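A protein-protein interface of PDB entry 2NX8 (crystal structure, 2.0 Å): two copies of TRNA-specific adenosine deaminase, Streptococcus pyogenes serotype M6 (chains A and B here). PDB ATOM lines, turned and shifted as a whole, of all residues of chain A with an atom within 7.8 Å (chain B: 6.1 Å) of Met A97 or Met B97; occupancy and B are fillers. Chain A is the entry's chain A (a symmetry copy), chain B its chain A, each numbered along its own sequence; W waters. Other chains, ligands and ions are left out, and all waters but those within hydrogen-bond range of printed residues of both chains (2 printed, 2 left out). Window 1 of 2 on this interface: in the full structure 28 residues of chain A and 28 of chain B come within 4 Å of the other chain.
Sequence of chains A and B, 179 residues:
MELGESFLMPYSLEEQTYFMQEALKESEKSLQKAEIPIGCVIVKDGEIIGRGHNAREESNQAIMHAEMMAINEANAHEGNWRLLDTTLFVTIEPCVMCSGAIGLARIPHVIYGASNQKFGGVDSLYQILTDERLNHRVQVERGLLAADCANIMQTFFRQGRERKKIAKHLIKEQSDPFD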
ATOM      1  N   GLN A  61      12.732   6.131 -15.766  1.00  0.00           N
ATOM      2  CA  GLN A  61      12.179   6.919 -16.867  1.00  0.00           C
ATOM      3  C   GLN A  61      12.804   8.313 -16.889  1.00  0.00           C
ATOM      4  O   GLN A  61      12.711   9.063 -15.916  1.00  0.00           O
ATOM      5  CB  GLN A  61      10.660   7.044 -16.720  1.00  0.00           C
ATOM      6  CG  GLN A  61       9.865   5.839 -17.219  1.00  0.00           C
ATOM      7  CD  GLN A  61       8.375   5.956 -16.921  1.00  0.00           C
ATOM      8  OE1 GLN A  61       7.903   5.506 -15.882  1.00  0.00           O
ATOM      9  NE2 GLN A  61       7.634   6.576 -17.830  1.00  0.00           N
ATOM     10  N   ALA A  62      13.429   8.657 -18.011  1.00  0.00           N
ATOM     11  CA  ALA A  62      14.089   9.949 -18.174  1.00  0.00           C
ATOM     12  C   ALA A  62      13.157  11.159 -18.157  1.00  0.00           C
ATOM     13  O   ALA A  62      13.590  12.267 -17.844  1.00  0.00           O
ATOM     14  CB  ALA A  62      14.897   9.953 -19.463  1.00  0.00           C
ATOM     15  N   ILE A  63      11.887  10.957 -18.492  1.00  0.00           N
ATOM     16  CA  ILE A  63      10.921  12.060 -18.532  1.00  0.00           C
ATOM     17  C   ILE A  63      10.133  12.207 -17.239  1.00  0.00           C
ATOM     18  O   ILE A  63       9.278  13.089 -17.138  1.00  0.00           O
ATOM     19  CB  ILE A  63       9.868  11.856 -19.637  1.00  0.00           C
ATOM     20  CG1 ILE A  63       8.887  10.764 -19.210  1.00  0.00           C
ATOM     21  CG2 ILE A  63      10.546  11.463 -20.952  1.00  0.00           C
ATOM     22  CD1 ILE A  63       7.689  10.598 -20.145  1.00  0.00           C
ATOM     23  N   MET A  64      10.423  11.357 -16.257  1.00  0.00           N
ATOM     24  CA  MET A  64       9.673  11.369 -15.010  1.00  0.00           C
ATOM     25  C   MET A  64       9.953  12.497 -14.024  1.00  0.00           C
ATOM     26  O   MET A  64      10.328  12.258 -12.867  1.00  0.00           O
ATOM     27  CB  MET A  64       9.813  10.018 -14.307  1.00  0.00           C
ATOM     28  CG  MET A  64       8.689   9.725 -13.326  1.00  0.00           C
ATOM     29  SD  MET A  64       7.067   9.995 -14.077  1.00  0.00           S
ATOM     30  CE  MET A  64       7.088   8.764 -15.370  1.00  0.00           C
ATOM     31  N   HIS A  65       9.774  13.728 -14.494  1.00  0.00           N
ATOM     32  CA  HIS A  65       9.933  14.896 -13.645  1.00  0.00           C
ATOM     33  C   HIS A  65       8.573  15.125 -13.016  1.00  0.00           C
ATOM     34  O   HIS A  65       7.567  14.593 -13.496  1.00  0.00           O
ATOM     35  CB  HIS A  65      10.338  16.123 -14.461  1.00  0.00           C
ATOM     36  CG  HIS A  65      11.797  16.177 -14.779  1.00  0.00           C
ATOM     37  ND1 HIS A  65      12.394  17.283 -15.341  1.00  0.00           N
ATOM     38  CD2 HIS A  65      12.785  15.270 -14.593  1.00  0.00           C
ATOM     39  CE1 HIS A  65      13.688  17.058 -15.487  1.00  0.00           C
ATOM     40  NE2 HIS A  65      13.951  15.842 -15.041  1.00  0.00           N
ATOM     41  N   ALA A  66       8.537  15.914 -11.943  1.00  0.00           N
ATOM     42  CA  ALA A  66       7.291  16.199 -11.239  1.00  0.00           C
ATOM     43  C   ALA A  66       6.164  16.699 -12.147  1.00  0.00           C
ATOM     44  O   ALA A  66       5.046  16.197 -12.079  1.00  0.00           O
ATOM     45  CB  ALA A  66       7.548  17.221 -10.113  1.00  0.00           C
ATOM     46  N   GLU A  67       6.458  17.689 -12.985  1.00  0.00           N
ATOM     47  CA  GLU A  67       5.445  18.256 -13.877  1.00  0.00           C
ATOM     48  C   GLU A  67       4.840  17.241 -14.840  1.00  0.00           C
ATOM     49  O   GLU A  67       3.633  17.266 -15.096  1.00  0.00           O
ATOM     50  CB  GLU A  67       6.024  19.414 -14.694  1.00  0.00           C
ATOM     51  CG  GLU A  67       6.699  20.497 -13.876  1.00  0.00           C
ATOM     52  CD  GLU A  67       8.177  20.218 -13.633  1.00  0.00           C
ATOM     53  OE1 GLU A  67       8.998  21.103 -13.949  1.00  0.00           O
ATOM     54  OE2 GLU A  67       8.517  19.130 -13.129  1.00  0.00           O
ATOM     55  N   MET A  68       5.682  16.355 -15.374  1.00  0.00           N
ATOM     56  CA  MET A  68       5.239  15.326 -16.319  1.00  0.00           C
ATOM     57  C   MET A  68       4.297  14.345 -15.637  1.00  0.00           C
ATOM     58  O   MET A  68       3.277  13.947 -16.206  1.00  0.00           O
ATOM     59  CB  MET A  68       6.446  14.565 -16.883  1.00  0.00           C
ATOM     60  CG  MET A  68       7.457  15.454 -17.594  1.00  0.00           C
ATOM     61  SD  MET A  68       6.711  16.387 -18.947  1.00  0.00           S
ATOM     62  CE  MET A  68       6.931  15.212 -20.320  1.00  0.00           C
ATOM     63  N   MET A  69       4.641  13.960 -14.412  1.00  0.00           N
ATOM     64  CA  MET A  69       3.814  13.031 -13.644  1.00  0.00           C
ATOM     65  C   MET A  69       2.462  13.680 -13.329  1.00  0.00           C
ATOM     66  O   MET A  69       1.410  13.042 -13.418  1.00  0.00           O
ATOM     67  CB  MET A  69       4.525  12.656 -12.341  1.00  0.00           C
ATOM     68  CG  MET A  69       3.846  11.538 -11.557  1.00  0.00           C
ATOM     69  SD  MET A  69       4.625  11.270  -9.951  1.00  0.00           S
ATOM     70  CE  MET A  69       6.068  10.317 -10.417  1.00  0.00           C
ATOM     71  N   ILE A  71       1.003  16.148 -14.999  1.00  0.00           N
ATOM     72  CA  ILE A  71       0.243  16.315 -16.232  1.00  0.00           C
ATOM     73  C   ILE A  71      -0.454  15.017 -16.616  1.00  0.00           C
ATOM     74  O   ILE A  71      -1.635  15.028 -16.969  1.00  0.00           O
ATOM     75  CB  ILE A  71       1.148  16.833 -17.373  1.00  0.00           C
ATOM     76  CG1 ILE A  71       1.532  18.284 -17.065  1.00  0.00           C
ATOM     77  CG2 ILE A  71       0.425  16.731 -18.725  1.00  0.00           C
ATOM     78  CD1 ILE A  71       2.427  18.949 -18.082  1.00  0.00           C
ATOM     79  N   PRO A  94      10.169  25.046 -14.161  1.00  0.00           N
ATOM     80  CA  PRO A  94      10.239  23.913 -15.096  1.00  0.00           C
ATOM     81  C   PRO A  94      11.392  23.967 -16.098  1.00  0.00           C
ATOM     82  O   PRO A  94      11.756  25.033 -16.608  1.00  0.00           O
ATOM     83  CB  PRO A  94       8.883  23.951 -15.794  1.00  0.00           C
ATOM     84  CG  PRO A  94       7.971  24.509 -14.721  1.00  0.00           C
ATOM     85  CD  PRO A  94       8.814  25.625 -14.141  1.00  0.00           C
ATOM     86  N   CYS A  95      11.959  22.799 -16.379  1.00  0.00           N
ATOM     87  CA  CYS A  95      13.046  22.695 -17.337  1.00  0.00           C
ATOM     88  C   CYS A  95      12.442  22.831 -18.740  1.00  0.00           C
ATOM     89  O   CYS A  95      11.241  23.077 -18.896  1.00  0.00           O
ATOM     90  CB  CYS A  95      13.740  21.338 -17.198  1.00  0.00           C
ATOM     91  SG  CYS A  95      12.773  19.946 -17.877  1.00  0.00           S
ATOM     92  N   VAL A  96      13.276  22.670 -19.756  1.00  0.00           N
ATOM     93  CA  VAL A  96      12.828  22.779 -21.140  1.00  0.00           C
ATOM     94  C   VAL A  96      11.778  21.728 -21.512  1.00  0.00           C
ATOM     95  O   VAL A  96      10.776  22.041 -22.154  1.00  0.00           O
ATOM     96  CB  VAL A  96      14.030  22.677 -22.098  1.00  0.00           C
ATOM     97  CG1 VAL A  96      13.555  22.508 -23.539  1.00  0.00           C
ATOM     98  CG2 VAL A  96      14.884  23.927 -21.971  1.00  0.00           C
ATOM     99  N   MET A  97      11.999  20.482 -21.110  1.00  0.00           N
ATOM    100  CA  MET A  97      11.044  19.425 -21.426  1.00  0.00           C
ATOM    101  C   MET A  97       9.664  19.686 -20.820  1.00  0.00           C
ATOM    102  O   MET A  97       8.642  19.605 -21.504  1.00  0.00           O
ATOM    103  CB  MET A  97      11.557  18.068 -20.929  1.00  0.00           C
ATOM    104  CG  MET A  97      10.555  16.947 -21.141  1.00  0.00           C
ATOM    105  SD  MET A  97      10.979  15.425 -20.295  1.00  0.00           S
ATOM    106  CE  MET A  97      10.875  16.003 -18.524  1.00  0.00           C
ATOM    107  N   CYS A  98       9.635  19.998 -19.529  1.00  0.00           N
ATOM    108  CA  CYS A  98       8.373  20.236 -18.851  1.00  0.00           C
ATOM    109  C   CYS A  98       7.670  21.486 -19.361  1.00  0.00           C
ATOM    110  O   CYS A  98       6.441  21.503 -19.492  1.00  0.00           O
ATOM    111  CB  CYS A  98       8.603  20.291 -17.337  1.00  0.00           C
ATOM    112  SG  CYS A  98       9.092  18.673 -16.643  1.00  0.00           S
ATOM    113  N   SER A  99       8.439  22.526 -19.664  1.00  0.00           N
ATOM    114  CA  SER A  99       7.856  23.753 -20.195  1.00  0.00           C
ATOM    115  C   SER A  99       7.139  23.410 -21.500  1.00  0.00           C
ATOM    116  O   SER A  99       5.994  23.812 -21.725  1.00  0.00           O
ATOM    117  CB  SER A  99       8.942  24.795 -20.468  1.00  0.00           C
ATOM    118  OG  SER A  99       9.551  25.234 -19.271  1.00  0.00           O
ATOM    119  N   GLY A 100       7.823  22.661 -22.360  1.00  0.00           N
ATOM    120  CA  GLY A 100       7.226  22.272 -23.624  1.00  0.00           C
ATOM    121  C   GLY A 100       5.951  21.484 -23.392  1.00  0.00           C
ATOM    122  O   GLY A 100       4.954  21.673 -24.089  1.00  0.00           O
ATOM    123  N   ALA A 101       5.983  20.594 -22.404  1.00  0.00           N
ATOM    124  CA  ALA A 101       4.830  19.768 -22.072  1.00  0.00           C
ATOM    125  C   ALA A 101       3.675  20.644 -21.579  1.00  0.00           C
ATOM    126  O   ALA A 101       2.527  20.446 -21.961  1.00  0.00           O
ATOM    127  CB  ALA A 101       5.213  18.751 -21.004  1.00  0.00           C
ATOM    128  N   ILE A 102       3.994  21.612 -20.727  1.00  0.00           N
ATOM    129  CA  ILE A 102       3.000  22.530 -20.185  1.00  0.00           C
ATOM    130  C   ILE A 102       2.300  23.278 -21.331  1.00  0.00           C
ATOM    131  O   ILE A 102       1.089  23.511 -21.297  1.00  0.00           O
ATOM    132  CB  ILE A 102       3.679  23.530 -19.219  1.00  0.00           C
ATOM    133  CG1 ILE A 102       4.169  22.774 -17.975  1.00  0.00           C
ATOM    134  CG2 ILE A 102       2.722  24.657 -18.851  1.00  0.00           C
ATOM    135  CD1 ILE A 102       5.016  23.609 -17.025  1.00  0.00           C
ATOM    136  N   GLY A 103       3.071  23.647 -22.348  1.00  0.00           N
ATOM    137  CA  GLY A 103       2.490  24.338 -23.485  1.00  0.00           C
ATOM    138  C   GLY A 103       1.568  23.426 -24.281  1.00  0.00           C
ATOM    139  O   GLY A 103       0.508  23.841 -24.743  1.00  0.00           O
ATOM    140  N   LEU A 104       1.971  22.171 -24.438  1.00  0.00           N
ATOM    141  CA  LEU A 104       1.176  21.203 -25.186  1.00  0.00           C
ATOM    142  C   LEU A 104      -0.137  20.855 -24.480  1.00  0.00           C
ATOM    143  O   LEU A 104      -1.124  20.497 -25.132  1.00  0.00           O
ATOM    144  CB  LEU A 104       1.992  19.928 -25.414  1.00  0.00           C
ATOM    145  CG  LEU A 104       3.179  20.037 -26.377  1.00  0.00           C
ATOM    146  CD1 LEU A 104       4.022  18.771 -26.284  1.00  0.00           C
ATOM    147  CD2 LEU A 104       2.676  20.254 -27.801  1.00  0.00           C
ATOM    148  N   ALA A 105      -0.142  20.955 -23.152  1.00  0.00           N
ATOM    149  CA  ALA A 105      -1.331  20.649 -22.352  1.00  0.00           C
ATOM    150  C   ALA A 105      -2.304  21.822 -22.331  1.00  0.00           C
ATOM    151  O   ALA A 105      -3.433  21.704 -21.846  1.00  0.00           O
ATOM    152  CB  ALA A 105      -0.925  20.287 -20.919  1.00  0.00           C
ATOM    153  N   PHE A 119      18.845  24.810 -15.609  1.00  0.00           N
ATOM    154  CA  PHE A 119      18.028  24.161 -16.631  1.00  0.00           C
ATOM    155  C   PHE A 119      16.673  24.834 -16.854  1.00  0.00           C
ATOM    156  O   PHE A 119      15.847  24.327 -17.610  1.00  0.00           O
ATOM    157  CB  PHE A 119      17.790  22.688 -16.263  1.00  0.00           C
ATOM    158  CG  PHE A 119      19.020  21.972 -15.759  1.00  0.00           C
ATOM    159  CD1 PHE A 119      19.353  21.998 -14.406  1.00  0.00           C
ATOM    160  CD2 PHE A 119      19.855  21.289 -16.638  1.00  0.00           C
ATOM    161  CE1 PHE A 119      20.498  21.354 -13.938  1.00  0.00           C
ATOM    162  CE2 PHE A 119      21.004  20.642 -16.179  1.00  0.00           C
ATOM    163  CZ  PHE A 119      21.326  20.675 -14.826  1.00  0.00           C
ATOM    164  N   GLY A 121      13.548  26.598 -18.124  1.00  0.00           N
ATOM    165  CA  GLY A 121      13.054  26.896 -19.456  1.00  0.00           C
ATOM    166  C   GLY A 121      11.926  27.910 -19.517  1.00  0.00           C
ATOM    167  O   GLY A 121      11.357  28.144 -20.581  1.00  0.00           O
ATOM    168  N   ILE A 128      10.047  29.563 -22.895  1.00  0.00           N
ATOM    169  CA  ILE A 128       9.118  28.735 -23.661  1.00  0.00           C
ATOM    170  C   ILE A 128       7.621  28.980 -23.433  1.00  0.00           C
ATOM    171  O   ILE A 128       6.840  28.954 -24.377  1.00  0.00           O
ATOM    172  CB  ILE A 128       9.413  27.231 -23.414  1.00  0.00           C
ATOM    173  CG1 ILE A 128      10.858  26.921 -23.820  1.00  0.00           C
ATOM    174  CG2 ILE A 128       8.450  26.363 -24.209  1.00  0.00           C
ATOM    175  CD1 ILE A 128      11.335  25.548 -23.399  1.00  0.00           C
ATOM    176  N   LEU A 134       5.566  29.763 -30.552  1.00  0.00           N
ATOM    177  CA  LEU A 134       4.791  28.598 -30.144  1.00  0.00           C
ATOM    178  C   LEU A 134       3.423  29.072 -29.675  1.00  0.00           C
ATOM    179  O   LEU A 134       2.551  28.278 -29.325  1.00  0.00           O
ATOM    180  CB  LEU A 134       5.517  27.844 -29.022  1.00  0.00           C
ATOM    181  CG  LEU A 134       6.852  27.193 -29.412  1.00  0.00           C
ATOM    182  CD1 LEU A 134       7.450  26.454 -28.232  1.00  0.00           C
ATOM    183  CD2 LEU A 134       6.622  26.230 -30.561  1.00  0.00           C
ATOM    184  N   HIS A 136       2.477  30.149 -27.056  1.00  0.00           N
ATOM    185  CA  HIS A 136       2.103  29.832 -25.690  1.00  0.00           C
ATOM    186  C   HIS A 136       1.851  31.182 -25.036  1.00  0.00           C
ATOM    187  O   HIS A 136       2.676  32.091 -25.141  1.00  0.00           O
ATOM    188  CB  HIS A 136       3.231  29.099 -24.960  1.00  0.00           C
ATOM    189  CG  HIS A 136       3.559  27.758 -25.537  1.00  0.00           C
ATOM    190  ND1 HIS A 136       2.605  26.933 -26.092  1.00  0.00           N
ATOM    191  CD2 HIS A 136       4.731  27.082 -25.612  1.00  0.00           C
ATOM    192  CE1 HIS A 136       3.174  25.807 -26.483  1.00  0.00           C
ATOM    193  NE2 HIS A 136       4.463  25.873 -26.203  1.00  0.00           N
ATOM    194  N   ALA B  62      -1.224  14.628 -23.013  1.00  0.00           N
ATOM    195  CA  ALA B  62      -0.604  15.735 -23.735  1.00  0.00           C
ATOM    196  C   ALA B  62       0.859  15.519 -24.120  1.00  0.00           C
ATOM    197  O   ALA B  62       1.344  16.133 -25.068  1.00  0.00           O
ATOM    198  CB  ALA B  62      -0.728  17.013 -22.919  1.00  0.00           C
ATOM    199  N   ILE B  63       1.561  14.657 -23.391  1.00  0.00           N
ATOM    200  CA  ILE B  63       2.980  14.402 -23.665  1.00  0.00           C
ATOM    201  C   ILE B  63       3.204  13.198 -24.568  1.00  0.00           C
ATOM    202  O   ILE B  63       4.351  12.863 -24.870  1.00  0.00           O
ATOM    203  CB  ILE B  63       3.764  14.103 -22.374  1.00  0.00           C
ATOM    204  CG1 ILE B  63       3.413  12.699 -21.880  1.00  0.00           C
ATOM    205  CG2 ILE B  63       3.427  15.134 -21.294  1.00  0.00           C
ATOM    206  CD1 ILE B  63       4.266  12.217 -20.706  1.00  0.00           C
ATOM    207  N   MET B  64       2.120  12.560 -25.000  1.00  0.00           N
ATOM    208  CA  MET B  64       2.233  11.354 -25.806  1.00  0.00           C
ATOM    209  C   MET B  64       2.638  11.511 -27.266  1.00  0.00           C
ATOM    210  O   MET B  64       1.913  11.094 -28.182  1.00  0.00           O
ATOM    211  CB  MET B  64       0.939  10.543 -25.711  1.00  0.00           C
ATOM    212  CG  MET B  64       1.121   9.070 -26.041  1.00  0.00           C
ATOM    213  SD  MET B  64       2.504   8.352 -25.124  1.00  0.00           S
ATOM    214  CE  MET B  64       1.925   8.537 -23.445  1.00  0.00           C
ATOM    215  N   HIS B  65       3.800  12.123 -27.476  1.00  0.00           N
ATOM    216  CA  HIS B  65       4.347  12.277 -28.814  1.00  0.00           C
ATOM    217  C   HIS B  65       5.160  11.022 -29.065  1.00  0.00           C
ATOM    218  O   HIS B  65       5.496  10.300 -28.121  1.00  0.00           O
ATOM    219  CB  HIS B  65       5.252  13.506 -28.905  1.00  0.00           C
ATOM    220  CG  HIS B  65       4.506  14.788 -29.080  1.00  0.00           C
ATOM    221  ND1 HIS B  65       5.134  15.979 -29.366  1.00  0.00           N
ATOM    222  CD2 HIS B  65       3.181  15.064 -29.032  1.00  0.00           C
ATOM    223  CE1 HIS B  65       4.230  16.935 -29.489  1.00  0.00           C
ATOM    224  NE2 HIS B  65       3.036  16.405 -29.290  1.00  0.00           N
ATOM    225  N   MET B  68       8.470  10.578 -26.996  1.00  0.00           N
ATOM    226  CA  MET B  68       8.225  10.317 -25.575  1.00  0.00           C
ATOM    227  C   MET B  68       7.864   8.855 -25.355  1.00  0.00           C
ATOM    228  O   MET B  68       8.333   8.223 -24.406  1.00  0.00           O
ATOM    229  CB  MET B  68       7.086  11.206 -25.058  1.00  0.00           C
ATOM    230  CG  MET B  68       7.345  12.697 -25.226  1.00  0.00           C
ATOM    231  SD  MET B  68       8.867  13.221 -24.410  1.00  0.00           S
ATOM    232  CE  MET B  68       8.234  13.620 -22.751  1.00  0.00           C
ATOM    233  N   CYS B  95       9.825  18.441 -31.272  1.00  0.00           N
ATOM    234  CA  CYS B  95       9.361  19.712 -30.744  1.00  0.00           C
ATOM    235  C   CYS B  95      10.214  20.043 -29.514  1.00  0.00           C
ATOM    236  O   CYS B  95      11.162  19.323 -29.183  1.00  0.00           O
ATOM    237  CB  CYS B  95       7.887  19.608 -30.344  1.00  0.00           C
ATOM    238  SG  CYS B  95       7.609  18.667 -28.804  1.00  0.00           S
ATOM    239  N   VAL B  96       9.874  21.132 -28.840  1.00  0.00           N
ATOM    240  CA  VAL B  96      10.609  21.558 -27.654  1.00  0.00           C
ATOM    241  C   VAL B  96      10.552  20.535 -26.516  1.00  0.00           C
ATOM    242  O   VAL B  96      11.565  20.244 -25.883  1.00  0.00           O
ATOM    243  CB  VAL B  96      10.077  22.918 -27.160  1.00  0.00           C
ATOM    244  CG1 VAL B  96      10.634  23.240 -25.776  1.00  0.00           C
ATOM    245  CG2 VAL B  96      10.469  24.002 -28.149  1.00  0.00           C
ATOM    246  N   MET B  97       9.373  19.984 -26.255  1.00  0.00           N
ATOM    247  CA  MET B  97       9.239  19.000 -25.187  1.00  0.00           C
ATOM    248  C   MET B  97      10.094  17.755 -25.430  1.00  0.00           C
ATOM    249  O   MET B  97      10.835  17.311 -24.551  1.00  0.00           O
ATOM    250  CB  MET B  97       7.774  18.574 -25.025  1.00  0.00           C
ATOM    251  CG  MET B  97       7.592  17.475 -23.993  1.00  0.00           C
ATOM    252  SD  MET B  97       5.961  16.733 -24.004  1.00  0.00           S
ATOM    253  CE  MET B  97       5.965  15.971 -25.707  1.00  0.00           C
ATOM    254  N   CYS B  98       9.988  17.191 -26.627  1.00  0.00           N
ATOM    255  CA  CYS B  98      10.735  15.987 -26.948  1.00  0.00           C
ATOM    256  C   CYS B  98      12.236  16.234 -26.991  1.00  0.00           C
ATOM    257  O   CYS B  98      13.022  15.386 -26.553  1.00  0.00           O
ATOM    258  CB  CYS B  98      10.219  15.396 -28.265  1.00  0.00           C
ATOM    259  SG  CYS B  98       8.518  14.743 -28.121  1.00  0.00           S
ATOM    260  N   SER B  99      12.640  17.393 -27.500  1.00  0.00           N
ATOM    261  CA  SER B  99      14.058  17.730 -27.546  1.00  0.00           C
ATOM    262  C   SER B  99      14.592  17.731 -26.115  1.00  0.00           C
ATOM    263  O   SER B  99      15.643  17.152 -25.824  1.00  0.00           O
ATOM    264  CB  SER B  99      14.266  19.113 -28.167  1.00  0.00           C
ATOM    265  OG  SER B  99      13.898  19.127 -29.532  1.00  0.00           O
ATOM    266  N   GLY B 100      13.858  18.386 -25.219  1.00  0.00           N
ATOM    267  CA  GLY B 100      14.274  18.435 -23.830  1.00  0.00           C
ATOM    268  C   GLY B 100      14.383  17.036 -23.256  1.00  0.00           C
ATOM    269  O   GLY B 100      15.315  16.727 -22.514  1.00  0.00           O
ATOM    270  N   ALA B 101      13.421  16.184 -23.600  1.00  0.00           N
ATOM    271  CA  ALA B 101      13.400  14.809 -23.120  1.00  0.00           C
ATOM    272  C   ALA B 101      14.613  14.043 -23.653  1.00  0.00           C
ATOM    273  O   ALA B 101      15.259  13.299 -22.923  1.00  0.00           O
ATOM    274  CB  ALA B 101      12.111  14.127 -23.561  1.00  0.00           C
ATOM    275  N   ILE B 102      14.913  14.234 -24.933  1.00  0.00           N
ATOM    276  CA  ILE B 102      16.048  13.581 -25.572  1.00  0.00           C
ATOM    277  C   ILE B 102      17.347  13.956 -24.841  1.00  0.00           C
ATOM    278  O   ILE B 102      18.238  13.123 -24.654  1.00  0.00           O
ATOM    279  CB  ILE B 102      16.124  13.996 -27.061  1.00  0.00           C
ATOM    280  CG1 ILE B 102      14.918  13.410 -27.810  1.00  0.00           C
ATOM    281  CG2 ILE B 102      17.441  13.546 -27.679  1.00  0.00           C
ATOM    282  CD1 ILE B 102      14.773  13.893 -29.246  1.00  0.00           C
ATOM    283  N   LEU B 104      17.574  14.871 -21.664  1.00  0.00           N
ATOM    284  CA  LEU B 104      17.531  14.268 -20.335  1.00  0.00           C
ATOM    285  C   LEU B 104      17.861  12.774 -20.361  1.00  0.00           C
ATOM    286  O   LEU B 104      18.364  12.225 -19.375  1.00  0.00           O
ATOM    287  CB  LEU B 104      16.147  14.480 -19.715  1.00  0.00           C
ATOM    288  CG  LEU B 104      15.784  15.916 -19.322  1.00  0.00           C
ATOM    289  CD1 LEU B 104      14.303  15.985 -18.973  1.00  0.00           C
ATOM    290  CD2 LEU B 104      16.644  16.367 -18.145  1.00  0.00           C
ATOM    291  N   ILE B 128      17.856  23.147 -28.990  1.00  0.00           N
ATOM    292  CA  ILE B 128      18.004  22.510 -27.683  1.00  0.00           C
ATOM    293  C   ILE B 128      19.022  21.368 -27.580  1.00  0.00           C
ATOM    294  O   ILE B 128      19.732  21.261 -26.587  1.00  0.00           O
ATOM    295  CB  ILE B 128      16.629  21.991 -27.183  1.00  0.00           C
ATOM    296  CG1 ILE B 128      15.643  23.160 -27.094  1.00  0.00           C
ATOM    297  CG2 ILE B 128      16.775  21.327 -25.823  1.00  0.00           C
ATOM    298  CD1 ILE B 128      14.209  22.739 -26.853  1.00  0.00           C
HETATM  299  O   HOH W   1      -1.003  17.420 -26.049  1.00  0.00           O
HETATM  300  O   HOH W   2      16.235  11.538 -17.069  1.00  0.00           O
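N of Met A97 sits close to SG of Cys A95.
The backbone carbonyl oxygen (O) of Gly A121 lies within hydrogen-bond range of the backbone NH (N) of Ile A128.
The side-chain sulfur (SG) of Cys B95 sits close to the backbone NH (N) of Met B97, 3.4 Å away.
Among the printed residues, pairs that only touch across the chains: Ala A62 with Leu B104 (3.9 Å), Ile A63 with Ile B63 (3.8 Å), Ile A63 with Met B68 (3.6 Å), His A65 with Leu B104 (3.7 Å), Met A68 with Ile B63 (3.6 Å), Met A68 with Met B68 (3.2 Å), Val A96 with Val B96 (3.8 Å), Val A96 with Ile B128 (3.4 Å), Met A97 with Met B97 (3.4 Å), Met A97 with Gly B100 (3.8 Å), Met A97 with Ala B101 (3.7 Å), Met A97 with Leu B104 (3.5 Å), Gly A100 with Met B97 (3.8 Å), Ala A101 with Met B97 (3.7 Å), Leu A104 with Ala B62 (3.9 Å), Leu A104 with His B65 (3.7 Å), Leu A104 with Met B97 (3.5 Å), Ala A105 with Ala B62 (3.7 Å), Ile A128 with Val B96 (3.4 Å) and Leu A134 with Val B96 (3.9 Å).
Met A97 touches just these residues of chain B: Met B97, Gly B100, Ala B101 and Leu B104.
Met B97 touches just these residues of chain A: Met A97 (3.4 Å), Gly A100 (3.8 Å), Ala A101 (3.7 Å) and Leu A104 (3.5 Å).
Of the printed residues of chain A, Met B68 touches Ile A63 and Met A68.
Printed residues of chain A within 4 Å of Ile B128: Val A96 (3.4 Å).
Printed residues of chain B within 4 Å of Leu A134: Val B96.
The nearest residue of chain A that does not touch Met B97 is Met A68 (4.1 Å).
The nearest printed residue of chain B that does not touch Val A96 is Gly B100 (4.1 Å).
Printed residues of chain B that touch a printed residue of chain A: Ala B62, Ile B63, His B65, Met B68, Val B96, Met B97, Gly B100, Ala B101, Leu B104 and Ile B128.
Hydrophobic or aromatic side chains of chain B within 4 Å of the printed part of chain A: Ala B62, Ile B63, His B65, Met B68, Val B96, Met B97, Ala B101, Leu B104 and Ile B128.
Hydrophobic or aromatic side chains of chain A within 4 Å of the printed part of chain B: Ile A63, His A65, Met A68, Val A96, Met A97, Ala A101, Leu A104, Ala A105, Ile A128 and Leu A134.
Among the printed residues, 20 pairs touch across the chains.
Among the printed residues, no Asp or Glu carboxylate lies within 4 Å of a Lys or Arg side-chain nitrogen of the other chain.
Ile A63 touches Met B68, and with the chains exchanged Met A68 touches Ile B63.
Met B68 touches its own counterpart, Met A68.
Val A96 touches Ile B128, and with the chains exchanged Ile A128 touches Val B96.
Met A97 touches Gly B100, and with the chains exchanged Gly A100 touches Met B97.
15 positions are printed for both chains.
Water W1 lies within hydrogen-bond range of the backbone carbonyl oxygen (O) of Ala B62 (2.9 Å) and the backbone carbonyl oxygen (O) of Leu A104 (3.2 Å).
Water W2 bridges the backbone carbonyl oxygen (O) of Ala A62 (2.9 Å) and the backbone carbonyl oxygen (O) of Leu B104 (3.2 Å).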
